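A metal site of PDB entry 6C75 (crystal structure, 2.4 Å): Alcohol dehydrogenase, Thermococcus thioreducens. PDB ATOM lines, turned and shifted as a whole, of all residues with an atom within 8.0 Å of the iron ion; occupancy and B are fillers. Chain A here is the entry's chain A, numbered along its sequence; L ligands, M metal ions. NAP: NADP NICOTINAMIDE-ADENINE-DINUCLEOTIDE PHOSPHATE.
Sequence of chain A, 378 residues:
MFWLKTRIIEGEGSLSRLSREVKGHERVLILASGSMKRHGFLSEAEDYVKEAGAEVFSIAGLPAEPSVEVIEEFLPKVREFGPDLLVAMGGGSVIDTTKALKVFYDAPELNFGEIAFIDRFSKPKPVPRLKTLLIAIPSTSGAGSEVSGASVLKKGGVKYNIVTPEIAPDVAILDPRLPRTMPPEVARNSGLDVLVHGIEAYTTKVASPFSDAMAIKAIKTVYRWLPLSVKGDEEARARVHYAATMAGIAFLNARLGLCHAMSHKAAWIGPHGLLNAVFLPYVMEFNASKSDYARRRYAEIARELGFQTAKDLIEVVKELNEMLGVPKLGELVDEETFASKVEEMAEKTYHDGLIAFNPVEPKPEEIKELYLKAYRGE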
ATOM      1  N   GLY A 142       2.127  -4.763   4.104  1.00  0.00           N
ATOM      2  CA  GLY A 142       3.419  -5.398   3.848  1.00  0.00           C
ATOM      3  C   GLY A 142       3.471  -6.767   4.499  1.00  0.00           C
ATOM      4  O   GLY A 142       2.708  -7.051   5.424  1.00  0.00           O
ATOM      5  N   ALA A 143       4.408  -7.595   4.047  1.00  0.00           N
ATOM      6  CA  ALA A 143       4.494  -8.983   4.482  1.00  0.00           C
ATOM      7  C   ALA A 143       5.411  -9.146   5.703  1.00  0.00           C
ATOM      8  O   ALA A 143       5.352 -10.170   6.378  1.00  0.00           O
ATOM      9  CB  ALA A 143       4.994  -9.865   3.351  1.00  0.00           C
ATOM     10  N   GLY A 144       6.285  -8.165   5.919  1.00  0.00           N
ATOM     11  CA  GLY A 144       7.186  -8.195   7.073  1.00  0.00           C
ATOM     12  C   GLY A 144       8.384  -9.115   6.849  1.00  0.00           C
ATOM     13  O   GLY A 144       9.206  -9.311   7.742  1.00  0.00           O
ATOM     14  N   VAL A 152       8.767 -18.321   2.183  1.00  0.00           N
ATOM     15  CA  VAL A 152       7.569 -19.121   1.930  1.00  0.00           C
ATOM     16  C   VAL A 152       7.463 -19.416   0.445  1.00  0.00           C
ATOM     17  O   VAL A 152       7.162 -18.525  -0.357  1.00  0.00           O
ATOM     18  CB  VAL A 152       6.298 -18.379   2.391  1.00  0.00           C
ATOM     19  CG1 VAL A 152       5.144 -19.351   2.536  1.00  0.00           C
ATOM     20  CG2 VAL A 152       6.544 -17.642   3.703  1.00  0.00           C
ATOM     21  N   ASN A 189      -4.812  -5.575   0.537  1.00  0.00           N
ATOM     22  CA  ASN A 189      -4.493  -6.971   0.847  1.00  0.00           C
ATOM     23  C   ASN A 189      -3.273  -7.073   1.745  1.00  0.00           C
ATOM     24  O   ASN A 189      -3.296  -7.797   2.745  1.00  0.00           O
ATOM     25  CB  ASN A 189      -4.254  -7.759  -0.440  1.00  0.00           C
ATOM     26  CG  ASN A 189      -5.528  -8.048  -1.197  1.00  0.00           C
ATOM     27  OD1 ASN A 189      -6.626  -7.707  -0.743  1.00  0.00           O
ATOM     28  ND2 ASN A 189      -5.396  -8.686  -2.348  1.00  0.00           N
ATOM     29  N   SER A 190      -2.199  -6.382   1.389  1.00  0.00           N
ATOM     30  CA  SER A 190      -0.988  -6.406   2.188  1.00  0.00           C
ATOM     31  C   SER A 190      -1.222  -5.684   3.522  1.00  0.00           C
ATOM     32  O   SER A 190      -0.637  -6.046   4.546  1.00  0.00           O
ATOM     33  CB  SER A 190       0.180  -5.781   1.420  1.00  0.00           C
ATOM     34  OG  SER A 190       0.034  -4.381   1.306  1.00  0.00           O
ATOM     35  N   LEU A 192      -4.047  -5.636   5.308  1.00  0.00           N
ATOM     36  CA  LEU A 192      -4.818  -6.486   6.225  1.00  0.00           C
ATOM     37  C   LEU A 192      -3.957  -7.628   6.758  1.00  0.00           C
ATOM     38  O   LEU A 192      -4.212  -8.152   7.839  1.00  0.00           O
ATOM     39  CB  LEU A 192      -6.065  -7.048   5.529  1.00  0.00           C
ATOM     40  CG  LEU A 192      -7.175  -6.047   5.217  1.00  0.00           C
ATOM     41  CD1 LEU A 192      -8.129  -6.618   4.178  1.00  0.00           C
ATOM     42  CD2 LEU A 192      -7.934  -5.672   6.488  1.00  0.00           C
ATOM     43  N   ASP A 193      -2.925  -7.994   6.005  1.00  0.00           N
ATOM     44  CA  ASP A 193      -1.906  -8.917   6.481  1.00  0.00           C
ATOM     45  C   ASP A 193      -1.215  -8.383   7.742  1.00  0.00           C
ATOM     46  O   ASP A 193      -1.079  -9.096   8.729  1.00  0.00           O
ATOM     47  CB  ASP A 193      -0.878  -9.139   5.371  1.00  0.00           C
ATOM     48  CG  ASP A 193      -0.305 -10.539   5.357  1.00  0.00           C
ATOM     49  OD1 ASP A 193      -0.795 -11.394   6.132  1.00  0.00           O
ATOM     50  OD2 ASP A 193       0.582 -10.791   4.519  1.00  0.00           O
ATOM     51  N   VAL A 194      -0.879  -7.098   7.728  1.00  0.00           N
ATOM     52  CA  VAL A 194      -0.354  -6.435   8.921  1.00  0.00           C
ATOM     53  C   VAL A 194      -1.269  -6.648  10.127  1.00  0.00           C
ATOM     54  O   VAL A 194      -0.800  -7.025  11.204  1.00  0.00           O
ATOM     55  CB  VAL A 194      -0.200  -4.915   8.685  1.00  0.00           C
ATOM     56  CG1 VAL A 194       0.327  -4.223   9.929  1.00  0.00           C
ATOM     57  CG2 VAL A 194       0.741  -4.651   7.520  1.00  0.00           C
ATOM     58  N   VAL A 196      -3.572  -8.837  10.718  1.00  0.00           N
ATOM     59  CA  VAL A 196      -3.652 -10.248  11.113  1.00  0.00           C
ATOM     60  C   VAL A 196      -2.368 -10.693  11.816  1.00  0.00           C
ATOM     61  O   VAL A 196      -2.425 -11.404  12.836  1.00  0.00           O
ATOM     62  CB  VAL A 196      -3.918 -11.158   9.898  1.00  0.00           C
ATOM     63  CG1 VAL A 196      -3.827 -12.626  10.301  1.00  0.00           C
ATOM     64  CG2 VAL A 196      -5.272 -10.869   9.287  1.00  0.00           C
ATOM     65  N   HIS A 197      -1.220 -10.300  11.271  1.00  0.00           N
ATOM     66  CA  HIS A 197       0.058 -10.510  11.956  1.00  0.00           C
ATOM     67  C   HIS A 197       0.016  -9.985  13.395  1.00  0.00           C
ATOM     68  O   HIS A 197       0.522 -10.647  14.318  1.00  0.00           O
ATOM     69  CB  HIS A 197       1.182  -9.809  11.211  1.00  0.00           C
ATOM     70  CG  HIS A 197       1.565 -10.482   9.925  1.00  0.00           C
ATOM     71  ND1 HIS A 197       2.162  -9.795   8.885  1.00  0.00           N
ATOM     72  CD2 HIS A 197       1.391 -11.754   9.505  1.00  0.00           C
ATOM     73  CE1 HIS A 197       2.318 -10.623   7.864  1.00  0.00           C
ATOM     74  NE2 HIS A 197       1.883 -11.814   8.222  1.00  0.00           N
ATOM     75  N   GLU A 200      -2.412 -12.092  15.635  1.00  0.00           N
ATOM     76  CA  GLU A 200      -1.900 -13.429  15.873  1.00  0.00           C
ATOM     77  C   GLU A 200      -0.667 -13.397  16.777  1.00  0.00           C
ATOM     78  O   GLU A 200      -0.576 -14.159  17.733  1.00  0.00           O
ATOM     79  CB  GLU A 200      -1.590 -14.139  14.550  1.00  0.00           C
ATOM     80  CG  GLU A 200      -2.828 -14.519  13.754  1.00  0.00           C
ATOM     81  CD  GLU A 200      -2.687 -15.855  13.049  1.00  0.00           C
ATOM     82  OE1 GLU A 200      -2.009 -15.904  12.007  1.00  0.00           O
ATOM     83  OE2 GLU A 200      -3.311 -16.846  13.505  1.00  0.00           O
ATOM     84  N   PHE A 251       6.240 -10.811  14.947  1.00  0.00           N
ATOM     85  CA  PHE A 251       6.003 -12.219  14.626  1.00  0.00           C
ATOM     86  C   PHE A 251       7.305 -12.967  14.282  1.00  0.00           C
ATOM     87  O   PHE A 251       7.393 -14.161  14.505  1.00  0.00           O
ATOM     88  CB  PHE A 251       4.927 -12.382  13.540  1.00  0.00           C
ATOM     89  CG  PHE A 251       5.425 -12.293  12.128  1.00  0.00           C
ATOM     90  CD1 PHE A 251       6.232 -13.287  11.593  1.00  0.00           C
ATOM     91  CD2 PHE A 251       4.873 -11.370  11.242  1.00  0.00           C
ATOM     92  CE1 PHE A 251       6.697 -13.201  10.290  1.00  0.00           C
ATOM     93  CE2 PHE A 251       5.315 -11.290   9.933  1.00  0.00           C
ATOM     94  CZ  PHE A 251       6.230 -12.201   9.458  1.00  0.00           C
ATOM     95  N   LEU A 256       3.380 -16.923  14.549  1.00  0.00           N
ATOM     96  CA  LEU A 256       1.985 -16.737  14.129  1.00  0.00           C
ATOM     97  C   LEU A 256       1.188 -18.015  14.409  1.00  0.00           C
ATOM     98  O   LEU A 256       1.704 -18.953  15.025  1.00  0.00           O
ATOM     99  CB  LEU A 256       1.927 -16.380  12.643  1.00  0.00           C
ATOM    100  CG  LEU A 256       2.616 -15.058  12.262  1.00  0.00           C
ATOM    101  CD1 LEU A 256       2.857 -14.957  10.758  1.00  0.00           C
ATOM    102  CD2 LEU A 256       1.811 -13.871  12.753  1.00  0.00           C
ATOM    103  N   HIS A 260      -2.783 -18.152   9.717  1.00  0.00           N
ATOM    104  CA  HIS A 260      -1.728 -18.202   8.724  1.00  0.00           C
ATOM    105  C   HIS A 260      -1.518 -19.618   8.213  1.00  0.00           C
ATOM    106  O   HIS A 260      -1.240 -19.817   7.029  1.00  0.00           O
ATOM    107  CB  HIS A 260      -0.424 -17.653   9.281  1.00  0.00           C
ATOM    108  CG  HIS A 260      -0.158 -16.229   8.888  1.00  0.00           C
ATOM    109  ND1 HIS A 260      -0.932 -15.182   9.341  1.00  0.00           N
ATOM    110  CD2 HIS A 260       0.681 -15.716   7.957  1.00  0.00           C
ATOM    111  CE1 HIS A 260      -0.552 -14.075   8.733  1.00  0.00           C
ATOM    112  NE2 HIS A 260       0.439 -14.366   7.916  1.00  0.00           N
ATOM    113  N   SER A 263      -4.372 -20.089   5.833  1.00  0.00           N
ATOM    114  CA  SER A 263      -4.076 -19.338   4.614  1.00  0.00           C
ATOM    115  C   SER A 263      -3.046 -20.025   3.728  1.00  0.00           C
ATOM    116  O   SER A 263      -3.121 -19.938   2.504  1.00  0.00           O
ATOM    117  CB  SER A 263      -3.582 -17.930   4.961  1.00  0.00           C
ATOM    118  OG  SER A 263      -4.583 -17.195   5.656  1.00  0.00           O
ATOM    119  N   HIS A 264      -2.019 -20.606   4.344  1.00  0.00           N
ATOM    120  CA  HIS A 264      -0.918 -21.205   3.595  1.00  0.00           C
ATOM    121  C   HIS A 264      -1.372 -22.438   2.807  1.00  0.00           C
ATOM    122  O   HIS A 264      -0.975 -22.613   1.658  1.00  0.00           O
ATOM    123  CB  HIS A 264       0.228 -21.586   4.546  1.00  0.00           C
ATOM    124  CG  HIS A 264       1.101 -20.431   4.916  1.00  0.00           C
ATOM    125  ND1 HIS A 264       2.306 -20.596   5.558  1.00  0.00           N
ATOM    126  CD2 HIS A 264       0.960 -19.102   4.725  1.00  0.00           C
ATOM    127  CE1 HIS A 264       2.848 -19.410   5.781  1.00  0.00           C
ATOM    128  NE2 HIS A 264       2.049 -18.487   5.286  1.00  0.00           N
ATOM    129  N   HIS A 272      -2.474 -13.993  -0.451  1.00  0.00           N
ATOM    130  CA  HIS A 272      -2.237 -14.306   0.960  1.00  0.00           C
ATOM    131  C   HIS A 272      -2.996 -13.369   1.902  1.00  0.00           C
ATOM    132  O   HIS A 272      -3.588 -13.823   2.884  1.00  0.00           O
ATOM    133  CB  HIS A 272      -0.739 -14.197   1.241  1.00  0.00           C
ATOM    134  CG  HIS A 272      -0.375 -14.487   2.660  1.00  0.00           C
ATOM    135  ND1 HIS A 272      -0.382 -15.757   3.183  1.00  0.00           N
ATOM    136  CD2 HIS A 272       0.012 -13.659   3.660  1.00  0.00           C
ATOM    137  CE1 HIS A 272       0.010 -15.711   4.443  1.00  0.00           C
ATOM    138  NE2 HIS A 272       0.274 -14.459   4.754  1.00  0.00           N
ATOM    139  N   GLY A 273      -2.863 -12.068   1.656  1.00  0.00           N
ATOM    140  CA  GLY A 273      -3.450 -11.057   2.542  1.00  0.00           C
ATOM    141  C   GLY A 273      -4.962 -11.140   2.570  1.00  0.00           C
ATOM    142  O   GLY A 273      -5.588 -11.018   3.629  1.00  0.00           O
ATOM    143  N   ASN A 276      -6.240 -14.486   4.595  1.00  0.00           N
ATOM    144  CA  ASN A 276      -6.097 -14.184   6.009  1.00  0.00           C
ATOM    145  C   ASN A 276      -7.215 -13.293   6.545  1.00  0.00           C
ATOM    146  O   ASN A 276      -7.723 -13.521   7.647  1.00  0.00           O
ATOM    147  CB  ASN A 276      -4.739 -13.508   6.261  1.00  0.00           C
ATOM    148  CG  ASN A 276      -3.632 -14.514   6.536  1.00  0.00           C
ATOM    149  OD1 ASN A 276      -3.723 -15.313   7.464  1.00  0.00           O
ATOM    150  ND2 ASN A 276      -2.622 -14.512   5.697  1.00  0.00           N
HETATM  151  PA  NAP L   1       3.668  -9.464  -3.297  1.00  0.00           P
HETATM  152  O1A NAP L   1       3.016 -10.818  -3.466  1.00  0.00           O
HETATM  153  O2A NAP L   1       5.169  -9.373  -3.088  1.00  0.00           O
HETATM  154  O5B NAP L   1       3.284  -8.604  -4.598  1.00  0.00           O
HETATM  155  C5B NAP L   1       1.904  -8.472  -4.933  1.00  0.00           C
HETATM  156  C4B NAP L   1       1.706  -7.574  -6.147  1.00  0.00           C
HETATM  157  O4B NAP L   1       1.887  -6.205  -5.787  1.00  0.00           O
HETATM  158  C3B NAP L   1       2.683  -7.868  -7.273  1.00  0.00           C
HETATM  159  O3B NAP L   1       1.983  -8.432  -8.390  1.00  0.00           O
HETATM  160  C2B NAP L   1       3.302  -6.538  -7.657  1.00  0.00           C
HETATM  161  O2B NAP L   1       3.190  -6.309  -9.056  1.00  0.00           O
HETATM  162  C1B NAP L   1       2.528  -5.498  -6.847  1.00  0.00           C
HETATM  163  N9A NAP L   1       3.383  -4.425  -6.296  1.00  0.00           N
HETATM  164  C8A NAP L   1       4.259  -4.544  -5.277  1.00  0.00           C
HETATM  165  N7A NAP L   1       4.778  -3.342  -4.952  1.00  0.00           N
HETATM  166  C5A NAP L   1       4.152  -2.405  -5.703  1.00  0.00           C
HETATM  167  C6A NAP L   1       4.261  -0.945  -5.904  1.00  0.00           C
HETATM  168  N6A NAP L   1       5.077  -0.181  -5.139  1.00  0.00           N
HETATM  169  N1A NAP L   1       3.478  -0.371  -6.854  1.00  0.00           N
HETATM  170  C2A NAP L   1       2.648  -1.109  -7.623  1.00  0.00           C
HETATM  171  N3A NAP L   1       2.529  -2.438  -7.518  1.00  0.00           N
HETATM  172  C4A NAP L   1       3.226  -3.133  -6.584  1.00  0.00           C
HETATM  173  O3  NAP L   1       2.895  -8.650  -2.113  1.00  0.00           O
HETATM  174  PN  NAP L   1       3.062  -8.944  -0.531  1.00  0.00           P
HETATM  175  O1N NAP L   1       4.162  -8.068   0.008  1.00  0.00           O
HETATM  176  O2N NAP L   1       1.711  -8.901   0.136  1.00  0.00           O
HETATM  177  O5D NAP L   1       3.631 -10.460  -0.556  1.00  0.00           O
HETATM  178  C5D NAP L   1       3.033 -11.550   0.115  1.00  0.00           C
HETATM  179  C4D NAP L   1       3.982 -12.740   0.009  1.00  0.00           C
HETATM  180  O4D NAP L   1       4.882 -12.737   1.131  1.00  0.00           O
HETATM  181  C3D NAP L   1       3.253 -14.083   0.010  1.00  0.00           C
HETATM  182  O3D NAP L   1       3.766 -14.939  -1.017  1.00  0.00           O
HETATM  183  C2D NAP L   1       3.517 -14.678   1.380  1.00  0.00           C
HETATM  184  O2D NAP L   1       3.717 -16.091   1.297  1.00  0.00           O
HETATM  185  C1D NAP L   1       4.777 -13.969   1.848  1.00  0.00           C
HETATM  186  N1N NAP L   1       4.785 -13.729   3.297  1.00  0.00           N
HETATM  187  C2N NAP L   1       5.964 -13.830   3.924  1.00  0.00           C
HETATM  188  C3N NAP L   1       6.058 -13.691   5.296  1.00  0.00           C
HETATM  189  C7N NAP L   1       7.405 -13.835   5.950  1.00  0.00           C
HETATM  190  O7N NAP L   1       7.570 -13.481   7.105  1.00  0.00           O
HETATM  191  N7N NAP L   1       8.410 -14.345   5.240  1.00  0.00           N
HETATM  192  C4N NAP L   1       4.908 -13.448   6.032  1.00  0.00           C
HETATM  193  C5N NAP L   1       3.695 -13.323   5.360  1.00  0.00           C
HETATM  194  C6N NAP L   1       3.656 -13.481   3.980  1.00  0.00           C
HETATM  195  P2B NAP L   1       4.441  -6.612 -10.035  1.00  0.00           P
HETATM  196  O1X NAP L   1       4.785  -8.049  -9.769  1.00  0.00           O
HETATM  197  O2X NAP L   1       3.891  -6.354 -11.418  1.00  0.00           O
HETATM  198  O3X NAP L   1       5.488  -5.620  -9.595  1.00  0.00           O
HETATM  199 FE    FE M   1       1.102 -12.788   6.476  1.00  0.00          FE
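OE1 of Glu 200 lies within hydrogen-bond range of ND1 of His 260, 3.0 Å away. The backbone carbonyl oxygen (O) of His 272 lies within hydrogen-bond range of the side-chain amide nitrogen (ND2) of Asn 276 (3.1 Å). OD1 of Asn 276 sits at hydrogen-bond distance from ND1 of His 260 (3.4 Å).
The nearest printed residue that does not touch the iron ion is Asn 276 (4.2 Å).
The iron ion is bound by a ring nitrogen (NE2) of His 197 (2.1 Å), a ring nitrogen (NE2) of His 260 (2.2 Å), the side-chain carboxylate (OD1) of Asp 193 (2.4 Å) and a ring nitrogen (NE2) of His 272 (2.5 Å). The iron ion has four donor atoms within binding distance. Slightly farther from the iron ion lies the side-chain carboxylate (OD2) of Asp 193 (2.8 Å).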
